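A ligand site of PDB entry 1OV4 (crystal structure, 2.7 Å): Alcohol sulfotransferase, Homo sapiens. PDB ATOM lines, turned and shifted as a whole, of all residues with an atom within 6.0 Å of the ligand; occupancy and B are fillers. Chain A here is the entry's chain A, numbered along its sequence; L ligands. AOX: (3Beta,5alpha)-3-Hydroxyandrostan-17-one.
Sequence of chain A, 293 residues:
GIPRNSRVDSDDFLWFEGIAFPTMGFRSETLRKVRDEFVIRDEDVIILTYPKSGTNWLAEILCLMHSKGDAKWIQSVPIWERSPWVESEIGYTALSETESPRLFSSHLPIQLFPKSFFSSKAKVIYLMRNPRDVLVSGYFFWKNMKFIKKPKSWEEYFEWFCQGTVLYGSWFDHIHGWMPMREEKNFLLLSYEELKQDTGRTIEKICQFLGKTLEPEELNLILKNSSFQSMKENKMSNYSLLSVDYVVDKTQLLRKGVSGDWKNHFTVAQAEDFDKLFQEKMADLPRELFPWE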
ATOM      1  N   PRO A  22      26.262  32.023 -26.078  1.00  0.00           N
ATOM      2  CA  PRO A  22      27.042  32.778 -25.102  1.00  0.00           C
ATOM      3  C   PRO A  22      28.435  32.992 -25.701  1.00  0.00           C
ATOM      4  O   PRO A  22      28.943  32.129 -26.403  1.00  0.00           O
ATOM      5  CB  PRO A  22      27.068  31.857 -23.885  1.00  0.00           C
ATOM      6  CG  PRO A  22      25.770  31.107 -24.003  1.00  0.00           C
ATOM      7  CD  PRO A  22      25.720  30.785 -25.479  1.00  0.00           C
ATOM      8  N   MET A  24      31.327  33.170 -24.154  1.00  0.00           N
ATOM      9  CA  MET A  24      32.287  32.270 -23.536  1.00  0.00           C
ATOM     10  C   MET A  24      31.844  30.828 -23.395  1.00  0.00           C
ATOM     11  O   MET A  24      30.664  30.546 -23.290  1.00  0.00           O
ATOM     12  CB  MET A  24      32.662  32.800 -22.151  1.00  0.00           C
ATOM     13  CG  MET A  24      33.313  34.174 -22.166  1.00  0.00           C
ATOM     14  SD  MET A  24      33.708  34.660 -20.500  1.00  0.00           S
ATOM     15  CE  MET A  24      32.024  34.748 -19.805  1.00  0.00           C
ATOM     16  N   GLY A  25      32.814  29.926 -23.405  1.00  0.00           N
ATOM     17  CA  GLY A  25      32.530  28.516 -23.257  1.00  0.00           C
ATOM     18  C   GLY A  25      32.020  27.840 -24.504  1.00  0.00           C
ATOM     19  O   GLY A  25      31.774  26.637 -24.505  1.00  0.00           O
ATOM     20  N   PHE A  26      31.874  28.612 -25.579  1.00  0.00           N
ATOM     21  CA  PHE A  26      31.392  28.067 -26.837  1.00  0.00           C
ATOM     22  C   PHE A  26      32.213  28.524 -28.017  1.00  0.00           C
ATOM     23  O   PHE A  26      32.404  29.721 -28.217  1.00  0.00           O
ATOM     24  CB  PHE A  26      29.947  28.489 -27.098  1.00  0.00           C
ATOM     25  CG  PHE A  26      28.978  28.047 -26.047  1.00  0.00           C
ATOM     26  CD1 PHE A  26      28.838  28.779 -24.875  1.00  0.00           C
ATOM     27  CD2 PHE A  26      28.181  26.925 -26.242  1.00  0.00           C
ATOM     28  CE1 PHE A  26      27.899  28.403 -23.921  1.00  0.00           C
ATOM     29  CE2 PHE A  26      27.246  26.540 -25.285  1.00  0.00           C
ATOM     30  CZ  PHE A  26      27.100  27.273 -24.136  1.00  0.00           C
ATOM     31  N   PRO A  51      16.464  26.889 -23.111  1.00  0.00           N
ATOM     32  CA  PRO A  51      16.923  27.442 -21.829  1.00  0.00           C
ATOM     33  C   PRO A  51      15.885  28.095 -20.892  1.00  0.00           C
ATOM     34  O   PRO A  51      15.054  28.887 -21.309  1.00  0.00           O
ATOM     35  CB  PRO A  51      18.064  28.394 -22.248  1.00  0.00           C
ATOM     36  CG  PRO A  51      17.770  28.704 -23.686  1.00  0.00           C
ATOM     37  CD  PRO A  51      17.225  27.424 -24.249  1.00  0.00           C
ATOM     38  N   LYS A  52      15.973  27.733 -19.615  1.00  0.00           N
ATOM     39  CA  LYS A  52      15.079  28.232 -18.561  1.00  0.00           C
ATOM     40  C   LYS A  52      13.732  27.557 -18.525  1.00  0.00           C
ATOM     41  O   LYS A  52      12.738  28.161 -18.133  1.00  0.00           O
ATOM     42  CB  LYS A  52      14.909  29.743 -18.658  1.00  0.00           C
ATOM     43  CG  LYS A  52      16.120  30.484 -18.162  1.00  0.00           C
ATOM     44  CD  LYS A  52      16.416  30.032 -16.755  1.00  0.00           C
ATOM     45  CE  LYS A  52      17.834  30.344 -16.375  1.00  0.00           C
ATOM     46  NZ  LYS A  52      18.146  29.735 -15.066  1.00  0.00           N
ATOM     47  N   THR A  55      15.548  22.570 -16.687  1.00  0.00           N
ATOM     48  CA  THR A  55      16.580  21.558 -16.904  1.00  0.00           C
ATOM     49  C   THR A  55      17.175  20.975 -15.629  1.00  0.00           C
ATOM     50  O   THR A  55      17.355  19.756 -15.499  1.00  0.00           O
ATOM     51  CB  THR A  55      17.739  22.126 -17.726  1.00  0.00           C
ATOM     52  OG1 THR A  55      17.226  23.062 -18.676  1.00  0.00           O
ATOM     53  CG2 THR A  55      18.457  21.007 -18.464  1.00  0.00           C
ATOM     54  N   ILE A  79      25.963  20.984 -11.561  1.00  0.00           N
ATOM     55  CA  ILE A  79      25.015  20.570 -12.596  1.00  0.00           C
ATOM     56  C   ILE A  79      25.774  20.232 -13.863  1.00  0.00           C
ATOM     57  O   ILE A  79      25.608  19.160 -14.435  1.00  0.00           O
ATOM     58  CB  ILE A  79      23.971  21.675 -12.912  1.00  0.00           C
ATOM     59  CG1 ILE A  79      24.665  22.974 -13.307  1.00  0.00           C
ATOM     60  CG2 ILE A  79      23.062  21.894 -11.711  1.00  0.00           C
ATOM     61  CD1 ILE A  79      23.706  24.079 -13.722  1.00  0.00           C
ATOM     62  N   TRP A  80      26.627  21.150 -14.302  1.00  0.00           N
ATOM     63  CA  TRP A  80      27.411  20.963 -15.520  1.00  0.00           C
ATOM     64  C   TRP A  80      28.305  19.722 -15.523  1.00  0.00           C
ATOM     65  O   TRP A  80      28.776  19.277 -16.573  1.00  0.00           O
ATOM     66  CB  TRP A  80      28.230  22.236 -15.813  1.00  0.00           C
ATOM     67  CG  TRP A  80      28.900  22.873 -14.621  1.00  0.00           C
ATOM     68  CD1 TRP A  80      29.985  22.414 -13.934  1.00  0.00           C
ATOM     69  CD2 TRP A  80      28.528  24.121 -13.998  1.00  0.00           C
ATOM     70  NE1 TRP A  80      30.332  23.306 -12.939  1.00  0.00           N
ATOM     71  CE2 TRP A  80      29.454  24.358 -12.953  1.00  0.00           C
ATOM     72  CE3 TRP A  80      27.521  25.060 -14.231  1.00  0.00           C
ATOM     73  CZ2 TRP A  80      29.394  25.484 -12.147  1.00  0.00           C
ATOM     74  CZ3 TRP A  80      27.457  26.194 -13.428  1.00  0.00           C
ATOM     75  CH2 TRP A  80      28.395  26.398 -12.395  1.00  0.00           C
ATOM     76  N   TRP A  85      26.598  19.990 -20.884  1.00  0.00           N
ATOM     77  CA  TRP A  85      25.958  20.487 -22.097  1.00  0.00           C
ATOM     78  C   TRP A  85      26.826  20.125 -23.301  1.00  0.00           C
ATOM     79  O   TRP A  85      27.868  20.743 -23.529  1.00  0.00           O
ATOM     80  CB  TRP A  85      25.779  22.005 -22.028  1.00  0.00           C
ATOM     81  CG  TRP A  85      24.601  22.430 -21.210  1.00  0.00           C
ATOM     82  CD1 TRP A  85      23.327  22.662 -21.670  1.00  0.00           C
ATOM     83  CD2 TRP A  85      24.568  22.681 -19.806  1.00  0.00           C
ATOM     84  NE1 TRP A  85      22.517  23.034 -20.630  1.00  0.00           N
ATOM     85  CE2 TRP A  85      23.255  23.050 -19.476  1.00  0.00           C
ATOM     86  CE3 TRP A  85      25.537  22.619 -18.794  1.00  0.00           C
ATOM     87  CZ2 TRP A  85      22.871  23.373 -18.162  1.00  0.00           C
ATOM     88  CZ3 TRP A  85      25.152  22.927 -17.489  1.00  0.00           C
ATOM     89  CH2 TRP A  85      23.828  23.304 -17.186  1.00  0.00           C
ATOM     90  N   GLU A  87      26.968  20.861 -26.250  1.00  0.00           N
ATOM     91  CA  GLU A  87      27.383  21.991 -27.090  1.00  0.00           C
ATOM     92  C   GLU A  87      28.491  22.872 -26.545  1.00  0.00           C
ATOM     93  O   GLU A  87      29.058  23.684 -27.270  1.00  0.00           O
ATOM     94  CB  GLU A  87      26.185  22.880 -27.403  1.00  0.00           C
ATOM     95  CG  GLU A  87      25.524  23.454 -26.162  1.00  0.00           C
ATOM     96  CD  GLU A  87      24.132  22.912 -25.949  1.00  0.00           C
ATOM     97  OE1 GLU A  87      23.925  21.698 -26.180  1.00  0.00           O
ATOM     98  OE2 GLU A  87      23.255  23.701 -25.525  1.00  0.00           O
ATOM     99  N   SER A  88      28.791  22.726 -25.260  1.00  0.00           N
ATOM    100  CA  SER A  88      29.810  23.535 -24.606  1.00  0.00           C
ATOM    101  C   SER A  88      31.208  22.919 -24.684  1.00  0.00           C
ATOM    102  O   SER A  88      31.362  21.696 -24.831  1.00  0.00           O
ATOM    103  CB  SER A  88      29.451  23.744 -23.147  1.00  0.00           C
ATOM    104  OG  SER A  88      29.432  22.507 -22.453  1.00  0.00           O
ATOM    105  N   GLU A  89      32.219  23.774 -24.565  1.00  0.00           N
ATOM    106  CA  GLU A  89      33.592  23.329 -24.594  1.00  0.00           C
ATOM    107  C   GLU A  89      33.776  22.306 -23.509  1.00  0.00           C
ATOM    108  O   GLU A  89      34.023  21.138 -23.782  1.00  0.00           O
ATOM    109  CB  GLU A  89      34.527  24.506 -24.360  1.00  0.00           C
ATOM    110  CG  GLU A  89      34.458  25.572 -25.434  1.00  0.00           C
ATOM    111  CD  GLU A  89      34.632  25.021 -26.827  1.00  0.00           C
ATOM    112  OE1 GLU A  89      35.624  24.303 -27.062  1.00  0.00           O
ATOM    113  OE2 GLU A  89      33.782  25.296 -27.692  1.00  0.00           O
ATOM    114  N   ILE A  90      33.637  22.744 -22.257  1.00  0.00           N
ATOM    115  CA  ILE A  90      33.793  21.842 -21.126  1.00  0.00           C
ATOM    116  C   ILE A  90      33.092  20.515 -21.372  1.00  0.00           C
ATOM    117  O   ILE A  90      33.739  19.478 -21.495  1.00  0.00           O
ATOM    118  CB  ILE A  90      33.221  22.447 -19.837  1.00  0.00           C
ATOM    119  CG1 ILE A  90      33.921  23.771 -19.527  1.00  0.00           C
ATOM    120  CG2 ILE A  90      33.383  21.465 -18.670  1.00  0.00           C
ATOM    121  CD1 ILE A  90      33.416  24.431 -18.256  1.00  0.00           C
ATOM    122  N   GLY A  91      31.758  20.576 -21.440  1.00  0.00           N
ATOM    123  CA  GLY A  91      30.934  19.415 -21.670  1.00  0.00           C
ATOM    124  C   GLY A  91      31.284  18.552 -22.866  1.00  0.00           C
ATOM    125  O   GLY A  91      31.434  17.335 -22.715  1.00  0.00           O
ATOM    126  N   HIS A 107      20.447  22.535 -25.224  1.00  0.00           N
ATOM    127  CA  HIS A 107      19.407  23.514 -25.529  1.00  0.00           C
ATOM    128  C   HIS A 107      19.318  23.668 -27.052  1.00  0.00           C
ATOM    129  O   HIS A 107      18.558  24.485 -27.576  1.00  0.00           O
ATOM    130  CB  HIS A 107      19.721  24.866 -24.907  1.00  0.00           C
ATOM    131  CG  HIS A 107      19.772  24.838 -23.407  1.00  0.00           C
ATOM    132  ND1 HIS A 107      18.839  24.168 -22.651  1.00  0.00           N
ATOM    133  CD2 HIS A 107      20.647  25.392 -22.538  1.00  0.00           C
ATOM    134  CE1 HIS A 107      19.138  24.309 -21.369  1.00  0.00           C
ATOM    135  NE2 HIS A 107      20.232  25.045 -21.277  1.00  0.00           N
ATOM    136  N   PHE A 141      17.802  36.328 -15.588  1.00  0.00           N
ATOM    137  CA  PHE A 141      18.962  35.449 -15.493  1.00  0.00           C
ATOM    138  C   PHE A 141      20.154  35.947 -16.261  1.00  0.00           C
ATOM    139  O   PHE A 141      21.292  35.985 -15.806  1.00  0.00           O
ATOM    140  CB  PHE A 141      18.656  34.075 -16.087  1.00  0.00           C
ATOM    141  CG  PHE A 141      19.907  33.231 -16.308  1.00  0.00           C
ATOM    142  CD1 PHE A 141      20.354  32.458 -15.268  1.00  0.00           C
ATOM    143  CD2 PHE A 141      20.600  33.200 -17.518  1.00  0.00           C
ATOM    144  CE1 PHE A 141      21.482  31.661 -15.401  1.00  0.00           C
ATOM    145  CE2 PHE A 141      21.723  32.411 -17.654  1.00  0.00           C
ATOM    146  CZ  PHE A 141      22.172  31.631 -16.601  1.00  0.00           C
ATOM    147  N   TRP A 142      19.843  36.303 -17.508  1.00  0.00           N
ATOM    148  CA  TRP A 142      20.798  36.791 -18.474  1.00  0.00           C
ATOM    149  C   TRP A 142      21.222  38.216 -18.191  1.00  0.00           C
ATOM    150  O   TRP A 142      22.321  38.633 -18.570  1.00  0.00           O
ATOM    151  CB  TRP A 142      20.198  36.699 -19.890  1.00  0.00           C
ATOM    152  CG  TRP A 142      19.895  35.295 -20.370  1.00  0.00           C
ATOM    153  CD1 TRP A 142      18.670  34.800 -20.760  1.00  0.00           C
ATOM    154  CD2 TRP A 142      20.821  34.206 -20.505  1.00  0.00           C
ATOM    155  NE1 TRP A 142      18.790  33.484 -21.118  1.00  0.00           N
ATOM    156  CE2 TRP A 142      20.100  33.089 -20.973  1.00  0.00           C
ATOM    157  CE3 TRP A 142      22.206  34.076 -20.269  1.00  0.00           C
ATOM    158  CZ2 TRP A 142      20.700  31.858 -21.231  1.00  0.00           C
ATOM    159  CZ3 TRP A 142      22.807  32.838 -20.515  1.00  0.00           C
ATOM    160  CH2 TRP A 142      22.047  31.746 -20.990  1.00  0.00           C
ATOM    161  N   MET A 145      24.278  38.171 -15.940  1.00  0.00           N
ATOM    162  CA  MET A 145      25.439  37.420 -16.433  1.00  0.00           C
ATOM    163  C   MET A 145      26.395  38.367 -17.119  1.00  0.00           C
ATOM    164  O   MET A 145      25.990  39.156 -17.976  1.00  0.00           O
ATOM    165  CB  MET A 145      24.990  36.349 -17.436  1.00  0.00           C
ATOM    166  CG  MET A 145      24.398  35.104 -16.810  1.00  0.00           C
ATOM    167  SD  MET A 145      25.659  34.043 -16.105  1.00  0.00           S
ATOM    168  CE  MET A 145      26.571  33.575 -17.607  1.00  0.00           C
ATOM    169  N   TYR A 168      20.004  31.124 -28.339  1.00  0.00           N
ATOM    170  CA  TYR A 168      19.360  29.875 -28.728  1.00  0.00           C
ATOM    171  C   TYR A 168      18.154  30.050 -29.658  1.00  0.00           C
ATOM    172  O   TYR A 168      17.452  29.098 -29.996  1.00  0.00           O
ATOM    173  CB  TYR A 168      18.982  29.063 -27.487  1.00  0.00           C
ATOM    174  CG  TYR A 168      20.183  28.496 -26.742  1.00  0.00           C
ATOM    175  CD1 TYR A 168      20.688  29.123 -25.595  1.00  0.00           C
ATOM    176  CD2 TYR A 168      20.817  27.344 -27.204  1.00  0.00           C
ATOM    177  CE1 TYR A 168      21.787  28.586 -24.912  1.00  0.00           C
ATOM    178  CE2 TYR A 168      21.907  26.809 -26.535  1.00  0.00           C
ATOM    179  CZ  TYR A 168      22.383  27.428 -25.397  1.00  0.00           C
ATOM    180  OH  TYR A 168      23.449  26.855 -24.730  1.00  0.00           O
HETATM  181  C1  AOX L   1      23.081  27.129 -20.736  1.00  0.00           C
HETATM  182  C2  AOX L   1      21.752  28.029 -20.744  1.00  0.00           C
HETATM  183  C3  AOX L   1      21.147  27.560 -19.326  1.00  0.00           C
HETATM  184  C4  AOX L   1      21.841  28.508 -18.208  1.00  0.00           C
HETATM  185  C5  AOX L   1      23.249  27.681 -18.121  1.00  0.00           C
HETATM  186  C6  AOX L   1      24.351  28.261 -17.059  1.00  0.00           C
HETATM  187  C7  AOX L   1      25.547  27.224 -16.893  1.00  0.00           C
HETATM  188  C8  AOX L   1      26.344  27.219 -18.296  1.00  0.00           C
HETATM  189  C9  AOX L   1      25.339  26.759 -19.473  1.00  0.00           C
HETATM  190  C10 AOX L   1      24.022  27.654 -19.614  1.00  0.00           C
HETATM  191  C11 AOX L   1      26.120  26.721 -20.876  1.00  0.00           C
HETATM  192  C12 AOX L   1      27.462  25.836 -20.813  1.00  0.00           C
HETATM  193  C13 AOX L   1      28.366  26.138 -19.550  1.00  0.00           C
HETATM  194  C14 AOX L   1      27.545  26.229 -18.276  1.00  0.00           C
HETATM  195  C15 AOX L   1      28.629  26.492 -17.202  1.00  0.00           C
HETATM  196  C16 AOX L   1      29.551  25.302 -17.547  1.00  0.00           C
HETATM  197  C17 AOX L   1      29.367  25.093 -19.066  1.00  0.00           C
HETATM  198  C18 AOX L   1      29.215  27.462 -19.948  1.00  0.00           C
HETATM  199  C19 AOX L   1      24.330  29.246 -19.794  1.00  0.00           C
HETATM  200  O3  AOX L   1      19.715  27.378 -19.047  1.00  0.00           O
HETATM  201  O17 AOX L   1      29.937  24.233 -19.683  1.00  0.00           O
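An oxygen (O3) of the ligand sits at hydrogen-bond distance from a ring nitrogen (NE2) of His 107 (3.3 Å).
An oxygen (O17) of the ligand lies within hydrogen-bond range of the side-chain hydroxyl of Ser 88 (3.3 Å).
The indole nitrogen (NE1) of Trp 85 lies within hydrogen-bond range of a ring nitrogen (NE2) of His 107 (3.1 Å).
The backbone NH (N) of His 107 lies within hydrogen-bond range of the side-chain carboxylate (OE2) of Glu 87 (3.1 Å).
The side-chain hydroxyl of Ser 88 is in hydrogen-bond range of the backbone carbonyl oxygen of Trp 85, at 2.6 Å.
The backbone NH (N) of Gly 91 lies within hydrogen-bond range of the side-chain hydroxyl (OG) of Ser 88.
Merely in contact with the ligand: Phe 26 (3.4 Å), Trp 80 (3.5 Å), Phe 141 (3.5 Å), Trp 142 (3.6 Å), Ile 90 (3.7 Å), Pro 51 (3.7 Å) and Lys 52 (3.8 Å).
Nine residues have an atom within 4 Å of the ligand: Phe 26, Pro 51, Lys 52, Trp 80, Ser 88, Ile 90, His 107, Phe 141 and Trp 142.
The nearest printed residue that does not touch the ligand is Tyr 168 (4.02 Å).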
